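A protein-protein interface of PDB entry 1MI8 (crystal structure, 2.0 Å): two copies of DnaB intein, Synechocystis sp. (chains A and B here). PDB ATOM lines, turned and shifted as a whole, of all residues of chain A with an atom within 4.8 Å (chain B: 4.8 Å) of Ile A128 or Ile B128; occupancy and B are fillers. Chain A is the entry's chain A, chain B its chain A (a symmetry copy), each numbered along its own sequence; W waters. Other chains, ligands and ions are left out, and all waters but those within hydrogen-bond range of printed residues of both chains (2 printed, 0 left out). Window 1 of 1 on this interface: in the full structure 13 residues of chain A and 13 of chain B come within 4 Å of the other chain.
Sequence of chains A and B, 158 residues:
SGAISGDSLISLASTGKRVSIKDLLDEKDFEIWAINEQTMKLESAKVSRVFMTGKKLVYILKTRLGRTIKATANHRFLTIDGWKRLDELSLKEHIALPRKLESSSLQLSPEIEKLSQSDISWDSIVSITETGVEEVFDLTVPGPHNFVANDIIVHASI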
ATOM      1  N   ILE A  60     -12.477  23.232  19.291  1.00  0.00           N
ATOM      2  CA  ILE A  60     -12.343  22.524  18.012  1.00  0.00           C
ATOM      3  C   ILE A  60     -11.729  21.162  18.211  1.00  0.00           C
ATOM      4  O   ILE A  60     -10.596  21.053  18.711  1.00  0.00           O
ATOM      5  CB  ILE A  60     -11.369  23.217  17.053  1.00  0.00           C
ATOM      6  CG1 ILE A  60     -11.893  24.592  16.671  1.00  0.00           C
ATOM      7  CG2 ILE A  60     -11.127  22.328  15.863  1.00  0.00           C
ATOM      8  CD1 ILE A  60     -10.845  25.461  15.870  1.00  0.00           C
ATOM      9  N   LEU A  61     -12.444  20.119  17.807  1.00  0.00           N
ATOM     10  CA  LEU A  61     -11.912  18.749  17.890  1.00  0.00           C
ATOM     11  C   LEU A  61     -11.640  18.365  16.426  1.00  0.00           C
ATOM     12  O   LEU A  61     -12.509  18.558  15.568  1.00  0.00           O
ATOM     13  CB  LEU A  61     -12.962  17.810  18.505  1.00  0.00           C
ATOM     14  CG  LEU A  61     -12.811  16.290  18.371  1.00  0.00           C
ATOM     15  CD1 LEU A  61     -13.842  15.593  19.261  1.00  0.00           C
ATOM     16  CD2 LEU A  61     -13.084  15.854  16.897  1.00  0.00           C
ATOM     17  N   LEU A  86     -15.659  15.921  25.653  1.00  0.00           N
ATOM     18  CA  LEU A  86     -14.584  16.504  24.859  1.00  0.00           C
ATOM     19  C   LEU A  86     -13.346  16.779  25.800  1.00  0.00           C
ATOM     20  O   LEU A  86     -12.172  16.504  25.437  1.00  0.00           O
ATOM     21  CB  LEU A  86     -15.080  17.839  24.203  1.00  0.00           C
ATOM     22  CG  LEU A  86     -14.144  18.472  23.160  1.00  0.00           C
ATOM     23  CD1 LEU A  86     -14.907  19.369  22.210  1.00  0.00           C
ATOM     24  CD2 LEU A  86     -13.077  19.229  23.874  1.00  0.00           C
ATOM     25  N   LEU A  89     -11.058  13.792  26.482  1.00  0.00           N
ATOM     26  CA  LEU A  89     -10.375  13.129  25.377  1.00  0.00           C
ATOM     27  C   LEU A  89      -8.911  13.481  25.361  1.00  0.00           C
ATOM     28  O   LEU A  89      -8.526  14.593  25.778  1.00  0.00           O
ATOM     29  CB  LEU A  89     -10.962  13.560  24.031  1.00  0.00           C
ATOM     30  CG  LEU A  89     -12.457  13.297  23.833  1.00  0.00           C
ATOM     31  CD1 LEU A  89     -12.965  13.947  22.504  1.00  0.00           C
ATOM     32  CD2 LEU A  89     -12.665  11.790  23.841  1.00  0.00           C
ATOM     33  N   SER A  90      -8.111  12.547  24.866  1.00  0.00           N
ATOM     34  CA  SER A  90      -6.669  12.747  24.707  1.00  0.00           C
ATOM     35  C   SER A  90      -6.322  12.278  23.310  1.00  0.00           C
ATOM     36  O   SER A  90      -7.125  11.638  22.624  1.00  0.00           O
ATOM     37  CB  SER A  90      -5.865  11.946  25.763  1.00  0.00           C
ATOM     38  OG  SER A  90      -6.426  10.648  25.917  1.00  0.00           O
ATOM     39  N   LEU A  91      -5.110  12.593  22.879  1.00  0.00           N
ATOM     40  CA  LEU A  91      -4.675  12.229  21.542  1.00  0.00           C
ATOM     41  C   LEU A  91      -4.521  10.731  21.339  1.00  0.00           C
ATOM     42  O   LEU A  91      -4.361  10.274  20.203  1.00  0.00           O
ATOM     43  CB  LEU A  91      -3.373  12.972  21.184  1.00  0.00           C
ATOM     44  CG  LEU A  91      -3.469  14.512  21.059  1.00  0.00           C
ATOM     45  CD1 LEU A  91      -2.683  14.925  19.857  1.00  0.00           C
ATOM     46  CD2 LEU A  91      -4.922  15.028  20.866  1.00  0.00           C
ATOM     47  N   ILE A 125      -7.735  11.184  17.222  1.00  0.00           N
ATOM     48  CA  ILE A 125      -7.881  12.591  17.458  1.00  0.00           C
ATOM     49  C   ILE A 125      -6.523  13.183  17.176  1.00  0.00           C
ATOM     50  O   ILE A 125      -5.517  12.649  17.625  1.00  0.00           O
ATOM     51  CB  ILE A 125      -8.241  12.886  18.928  1.00  0.00           C
ATOM     52  CG1 ILE A 125      -9.591  12.221  19.260  1.00  0.00           C
ATOM     53  CG2 ILE A 125      -8.378  14.407  19.124  1.00  0.00           C
ATOM     54  CD1 ILE A 125      -9.802  12.026  20.712  1.00  0.00           C
ATOM     55  N   VAL A 126      -6.483  14.286  16.418  1.00  0.00           N
ATOM     56  CA  VAL A 126      -5.212  14.941  16.159  1.00  0.00           C
ATOM     57  C   VAL A 126      -5.188  16.359  16.736  1.00  0.00           C
ATOM     58  O   VAL A 126      -4.118  16.987  16.808  1.00  0.00           O
ATOM     59  CB  VAL A 126      -4.851  14.986  14.649  1.00  0.00           C
ATOM     60  CG1 VAL A 126      -4.771  13.544  14.130  1.00  0.00           C
ATOM     61  CG2 VAL A 126      -5.833  15.864  13.852  1.00  0.00           C
ATOM     62  N   SER A 127      -6.353  16.869  17.102  1.00  0.00           N
ATOM     63  CA  SER A 127      -6.403  18.206  17.692  1.00  0.00           C
ATOM     64  C   SER A 127      -7.625  18.491  18.557  1.00  0.00           C
ATOM     65  O   SER A 127      -8.745  18.082  18.242  1.00  0.00           O
ATOM     66  CB  SER A 127      -6.299  19.306  16.595  1.00  0.00           C
ATOM     67  OG  SER A 127      -5.988  20.538  17.240  1.00  0.00           O
ATOM     68  N   ILE A 128      -7.382  19.203  19.656  1.00  0.00           N
ATOM     69  CA  ILE A 128      -8.410  19.621  20.587  1.00  0.00           C
ATOM     70  C   ILE A 128      -7.910  20.971  21.037  1.00  0.00           C
ATOM     71  O   ILE A 128      -6.835  21.072  21.696  1.00  0.00           O
ATOM     72  CB  ILE A 128      -8.508  18.716  21.830  1.00  0.00           C
ATOM     73  CG1 ILE A 128      -8.503  17.224  21.453  1.00  0.00           C
ATOM     74  CG2 ILE A 128      -9.851  18.984  22.548  1.00  0.00           C
ATOM     75  CD1 ILE A 128      -8.312  16.317  22.714  1.00  0.00           C
ATOM     76  N   THR A 129      -8.622  22.019  20.649  1.00  0.00           N
ATOM     77  CA  THR A 129      -8.182  23.348  21.033  1.00  0.00           C
ATOM     78  C   THR A 129      -9.350  24.303  21.352  1.00  0.00           C
ATOM     79  O   THR A 129     -10.341  24.338  20.637  1.00  0.00           O
ATOM     80  CB  THR A 129      -7.322  23.980  19.942  1.00  0.00           C
ATOM     81  OG1 THR A 129      -8.167  24.671  19.053  1.00  0.00           O
ATOM     82  CG2 THR A 129      -6.556  22.942  19.150  1.00  0.00           C
ATOM     83  N   GLU A 130      -9.249  25.020  22.463  1.00  0.00           N
ATOM     84  CA  GLU A 130     -10.281  25.963  22.865  1.00  0.00           C
ATOM     85  C   GLU A 130     -10.310  27.091  21.800  1.00  0.00           C
ATOM     86  O   GLU A 130      -9.253  27.505  21.330  1.00  0.00           O
ATOM     87  CB  GLU A 130      -9.909  26.531  24.232  1.00  0.00           C
ATOM     88  CG  GLU A 130     -10.936  27.501  24.850  1.00  0.00           C
ATOM     89  CD  GLU A 130     -10.311  28.308  25.972  1.00  0.00           C
ATOM     90  OE1 GLU A 130     -10.065  29.511  25.742  1.00  0.00           O
ATOM     91  OE2 GLU A 130     -10.049  27.726  27.047  1.00  0.00           O
ATOM     92  N   ILE B  60       1.973  20.483  19.486  1.00  0.00           N
ATOM     93  CA  ILE B  60       1.952  21.748  20.230  1.00  0.00           C
ATOM     94  C   ILE B  60       1.043  21.656  21.428  1.00  0.00           C
ATOM     95  O   ILE B  60      -0.164  21.399  21.279  1.00  0.00           O
ATOM     96  CB  ILE B  60       1.354  22.901  19.416  1.00  0.00           C
ATOM     97  CG1 ILE B  60       2.216  23.192  18.198  1.00  0.00           C
ATOM     98  CG2 ILE B  60       1.174  24.099  20.309  1.00  0.00           C
ATOM     99  CD1 ILE B  60       1.551  24.208  17.188  1.00  0.00           C
ATOM    100  N   LEU B  61       1.593  21.884  22.614  1.00  0.00           N
ATOM    101  CA  LEU B  61       0.782  21.888  23.844  1.00  0.00           C
ATOM    102  C   LEU B  61       0.733  23.369  24.253  1.00  0.00           C
ATOM    103  O   LEU B  61       1.776  24.031  24.290  1.00  0.00           O
ATOM    104  CB  LEU B  61       1.472  21.051  24.933  1.00  0.00           C
ATOM    105  CG  LEU B  61       1.039  21.186  26.399  1.00  0.00           C
ATOM    106  CD1 LEU B  61       1.706  20.089  27.231  1.00  0.00           C
ATOM    107  CD2 LEU B  61       1.504  22.563  26.968  1.00  0.00           C
ATOM    108  N   LEU B  86       2.244  13.466  26.885  1.00  0.00           N
ATOM    109  CA  LEU B  86       1.492  14.476  26.149  1.00  0.00           C
ATOM    110  C   LEU B  86       0.177  13.817  25.577  1.00  0.00           C
ATOM    111  O   LEU B  86      -0.932  14.410  25.634  1.00  0.00           O
ATOM    112  CB  LEU B  86       2.374  15.039  24.981  1.00  0.00           C
ATOM    113  CG  LEU B  86       1.816  16.266  24.239  1.00  0.00           C
ATOM    114  CD1 LEU B  86       2.922  17.054  23.571  1.00  0.00           C
ATOM    115  CD2 LEU B  86       0.809  15.802  23.244  1.00  0.00           C
ATOM    116  N   LEU B  89      -2.769  13.568  28.003  1.00  0.00           N
ATOM    117  CA  LEU B  89      -3.340  14.778  28.582  1.00  0.00           C
ATOM    118  C   LEU B  89      -4.668  15.103  27.948  1.00  0.00           C
ATOM    119  O   LEU B  89      -4.889  14.796  26.758  1.00  0.00           O
ATOM    120  CB  LEU B  89      -2.421  15.981  28.359  1.00  0.00           C
ATOM    121  CG  LEU B  89      -1.004  15.861  28.926  1.00  0.00           C
ATOM    122  CD1 LEU B  89      -0.119  17.068  28.471  1.00  0.00           C
ATOM    123  CD2 LEU B  89      -1.119  15.782  30.441  1.00  0.00           C
ATOM    124  N   SER B  90      -5.528  15.735  28.732  1.00  0.00           N
ATOM    125  CA  SER B  90      -6.837  16.194  28.260  1.00  0.00           C
ATOM    126  C   SER B  90      -6.989  17.623  28.734  1.00  0.00           C
ATOM    127  O   SER B  90      -6.216  18.116  29.561  1.00  0.00           O
ATOM    128  CB  SER B  90      -7.982  15.312  28.820  1.00  0.00           C
ATOM    129  OG  SER B  90      -7.745  15.022  30.192  1.00  0.00           O
ATOM    130  N   LEU B  91      -7.999  18.301  28.211  1.00  0.00           N
ATOM    131  CA  LEU B  91      -8.225  19.693  28.561  1.00  0.00           C
ATOM    132  C   LEU B  91      -8.642  19.895  30.009  1.00  0.00           C
ATOM    133  O   LEU B  91      -8.665  21.032  30.493  1.00  0.00           O
ATOM    134  CB  LEU B  91      -9.247  20.326  27.598  1.00  0.00           C
ATOM    135  CG  LEU B  91      -8.812  20.457  26.118  1.00  0.00           C
ATOM    136  CD1 LEU B  91      -9.240  21.803  25.631  1.00  0.00           C
ATOM    137  CD2 LEU B  91      -7.275  20.355  25.913  1.00  0.00           C
ATOM    138  N   ILE B 125      -4.651  23.266  30.454  1.00  0.00           N
ATOM    139  CA  ILE B 125      -4.268  23.031  29.092  1.00  0.00           C
ATOM    140  C   ILE B 125      -5.389  23.599  28.260  1.00  0.00           C
ATOM    141  O   ILE B 125      -6.553  23.358  28.555  1.00  0.00           O
ATOM    142  CB  ILE B 125      -4.153  21.524  28.786  1.00  0.00           C
ATOM    143  CG1 ILE B 125      -3.064  20.907  29.685  1.00  0.00           C
ATOM    144  CG2 ILE B 125      -3.747  21.332  27.314  1.00  0.00           C
ATOM    145  CD1 ILE B 125      -3.191  19.439  29.829  1.00  0.00           C
ATOM    146  N   VAL B 126      -5.049  24.369  27.219  1.00  0.00           N
ATOM    147  CA  VAL B 126      -6.079  24.897  26.342  1.00  0.00           C
ATOM    148  C   VAL B 126      -5.923  24.363  24.915  1.00  0.00           C
ATOM    149  O   VAL B 126      -6.834  24.526  24.083  1.00  0.00           O
ATOM    150  CB  VAL B 126      -6.116  26.450  26.317  1.00  0.00           C
ATOM    151  CG1 VAL B 126      -6.388  26.947  27.743  1.00  0.00           C
ATOM    152  CG2 VAL B 126      -4.835  27.042  25.701  1.00  0.00           C
ATOM    153  N   SER B 127      -4.775  23.774  24.626  1.00  0.00           N
ATOM    154  CA  SER B 127      -4.568  23.211  23.291  1.00  0.00           C
ATOM    155  C   SER B 127      -3.510  22.117  23.203  1.00  0.00           C
ATOM    156  O   SER B 127      -2.459  22.186  23.845  1.00  0.00           O
ATOM    157  CB  SER B 127      -4.222  24.326  22.261  1.00  0.00           C
ATOM    158  OG  SER B 127      -4.393  23.782  20.955  1.00  0.00           O
ATOM    159  N   ILE B 128      -3.814  21.106  22.392  1.00  0.00           N
ATOM    160  CA  ILE B 128      -2.928  19.990  22.131  1.00  0.00           C
ATOM    161  C   ILE B 128      -3.216  19.678  20.684  1.00  0.00           C
ATOM    162  O   ILE B 128      -4.356  19.258  20.332  1.00  0.00           O
ATOM    163  CB  ILE B 128      -3.268  18.737  22.961  1.00  0.00           C
ATOM    164  CG1 ILE B 128      -3.506  19.080  24.442  1.00  0.00           C
ATOM    165  CG2 ILE B 128      -2.069  17.762  22.922  1.00  0.00           C
ATOM    166  CD1 ILE B 128      -4.128  17.869  25.215  1.00  0.00           C
ATOM    167  N   THR B 129      -2.240  19.930  19.824  1.00  0.00           N
ATOM    168  CA  THR B 129      -2.463  19.670  18.413  1.00  0.00           C
ATOM    169  C   THR B 129      -1.210  19.134  17.692  1.00  0.00           C
ATOM    170  O   THR B 129      -0.112  19.628  17.898  1.00  0.00           O
ATOM    171  CB  THR B 129      -2.939  20.927  17.690  1.00  0.00           C
ATOM    172  OG1 THR B 129      -1.811  21.634  17.236  1.00  0.00           O
ATOM    173  CG2 THR B 129      -3.730  21.841  18.602  1.00  0.00           C
ATOM    174  N   GLU B 130      -1.380  18.081  16.903  1.00  0.00           N
ATOM    175  CA  GLU B 130      -0.276  17.492  16.161  1.00  0.00           C
ATOM    176  C   GLU B 130       0.198  18.548  15.129  1.00  0.00           C
ATOM    177  O   GLU B 130      -0.636  19.234  14.542  1.00  0.00           O
ATOM    178  CB  GLU B 130      -0.786  16.242  15.449  1.00  0.00           C
ATOM    179  CG  GLU B 130       0.276  15.442  14.668  1.00  0.00           C
ATOM    180  CD  GLU B 130      -0.379  14.490  13.686  1.00  0.00           C
ATOM    181  OE1 GLU B 130      -0.320  14.788  12.474  1.00  0.00           O
ATOM    182  OE2 GLU B 130      -0.965  13.482  14.138  1.00  0.00           O
HETATM  183  O   HOH W   1      -3.478  14.296  24.546  1.00  0.00           O
HETATM  184  O   HOH W   2      -9.541  17.040  26.121  1.00  0.00           O
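Water W1 lies within hydrogen-bond range of the backbone carbonyl oxygen (O) of Leu B89, the backbone carbonyl oxygen (O) of Leu B86 and the backbone NH (N) of Leu A91.
Water W2 lies within hydrogen-bond range of the backbone carbonyl oxygen (O) of Leu A89 (2.7 Å), the backbone carbonyl oxygen (O) of Leu A86 (2.8 Å) and the backbone NH (N) of Leu B91 (2.9 Å).
Leu B89 touches its own counterpart, Leu A89.
Leu A89 touches Ser B90, and with the chains exchanged Ser A90 touches Leu B89.
Val A126 touches Thr B129, and with the chains exchanged Thr A129 touches Val B126.
Ser A127 touches Ile B128, and with the chains exchanged Ile A128 touches Ser B127.
N of Glu A130 lies within hydrogen-bond range of O of Val B126 (2.9 Å).
The backbone carbonyl oxygen (O) of Val A126 sits at hydrogen-bond distance from the backbone NH (N) of Glu B130 (3.0 Å).
The backbone carbonyl oxygen (O) of Ile A128 lies within hydrogen-bond range of the backbone NH (N) of Ile B128 (3.1 Å).
O of Leu B89 touches O of Leu A89 (3.8 Å).
Leu A89 touches Ser B90 (O to CB, 3.2 Å).
Ser A90 touches Leu B89 (CB to O, 3.2 Å).
CG of Leu A91 touches CG2 of Ile B128, at 3.999 Å.
Val A126 touches Thr B129 (O to CA, 3.5 Å).
CA of Ser A127 touches O of Ile B128 (3.5 Å).
Thr B129 touches Ser A127 (CG2 to OG, 2.9 Å).
Leu B91 touches Ile A128.
Thr A129 touches Ser B127.
Thr A129 touches Thr B129 (CG2 to CG2, 3.1 Å).
Of the printed residues of chain B, Leu A91 touches Ile B128.
Ile A125 touches none of the printed residues of chain B.
Printed residues of chain B within 4 Å of Ser A127: Ile B128 and Thr B129.
Printed residues of chain B within 4 Å of Ile A128: Leu B91 (3.999 Å), Ser B127 (3.5 Å) and Ile B128 (3.1 Å).
Of the printed residues of chain B, Glu A130 touches Val B126 (2.9 Å).
Leu B86 touches none of the printed residues of chain A.
Of the printed residues of chain A, Ser B127 touches Ile A128 (3.5 Å) and Thr A129 (2.9 Å).
Printed residues of chain A within 4 Å of Ile B128: Leu A91 (3.999 Å), Ser A127 (3.5 Å) and Ile A128 (3.1 Å).
Of the printed residues of chain A, Glu B130 touches Val A126.
The nearest printed residue of chain B that does not touch Ile A128 is Val B126 (4.2 Å).
The nearest printed residue of chain A that does not touch Ser B127 is Glu A130 (5.1 Å).
O of Thr B129 lies within hydrogen-bond range of N of Ile B60.
N of Ile A60 sits at hydrogen-bond distance from O of Thr A129, at 2.8 Å.
Of the 12 printed residues of chain B, 8 touch a printed residue of chain A.
Hydrophobic or aromatic side chains of chain B within 4 Å of the printed part of chain A: Leu B91, Val B126 and Ile B128.
Of the 12 printed residues of chain A, 8 touch a printed residue of chain B.
Printed residues of chain A that touch a printed residue of chain B: Leu A89, Ser A90, Leu A91, Val A126, Ser A127, Ile A128, Thr A129 and Glu A130.
Among the printed residues, no Asp or Glu carboxylate lies within 4 Å of a Lys or Arg side-chain nitrogen of the other chain.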
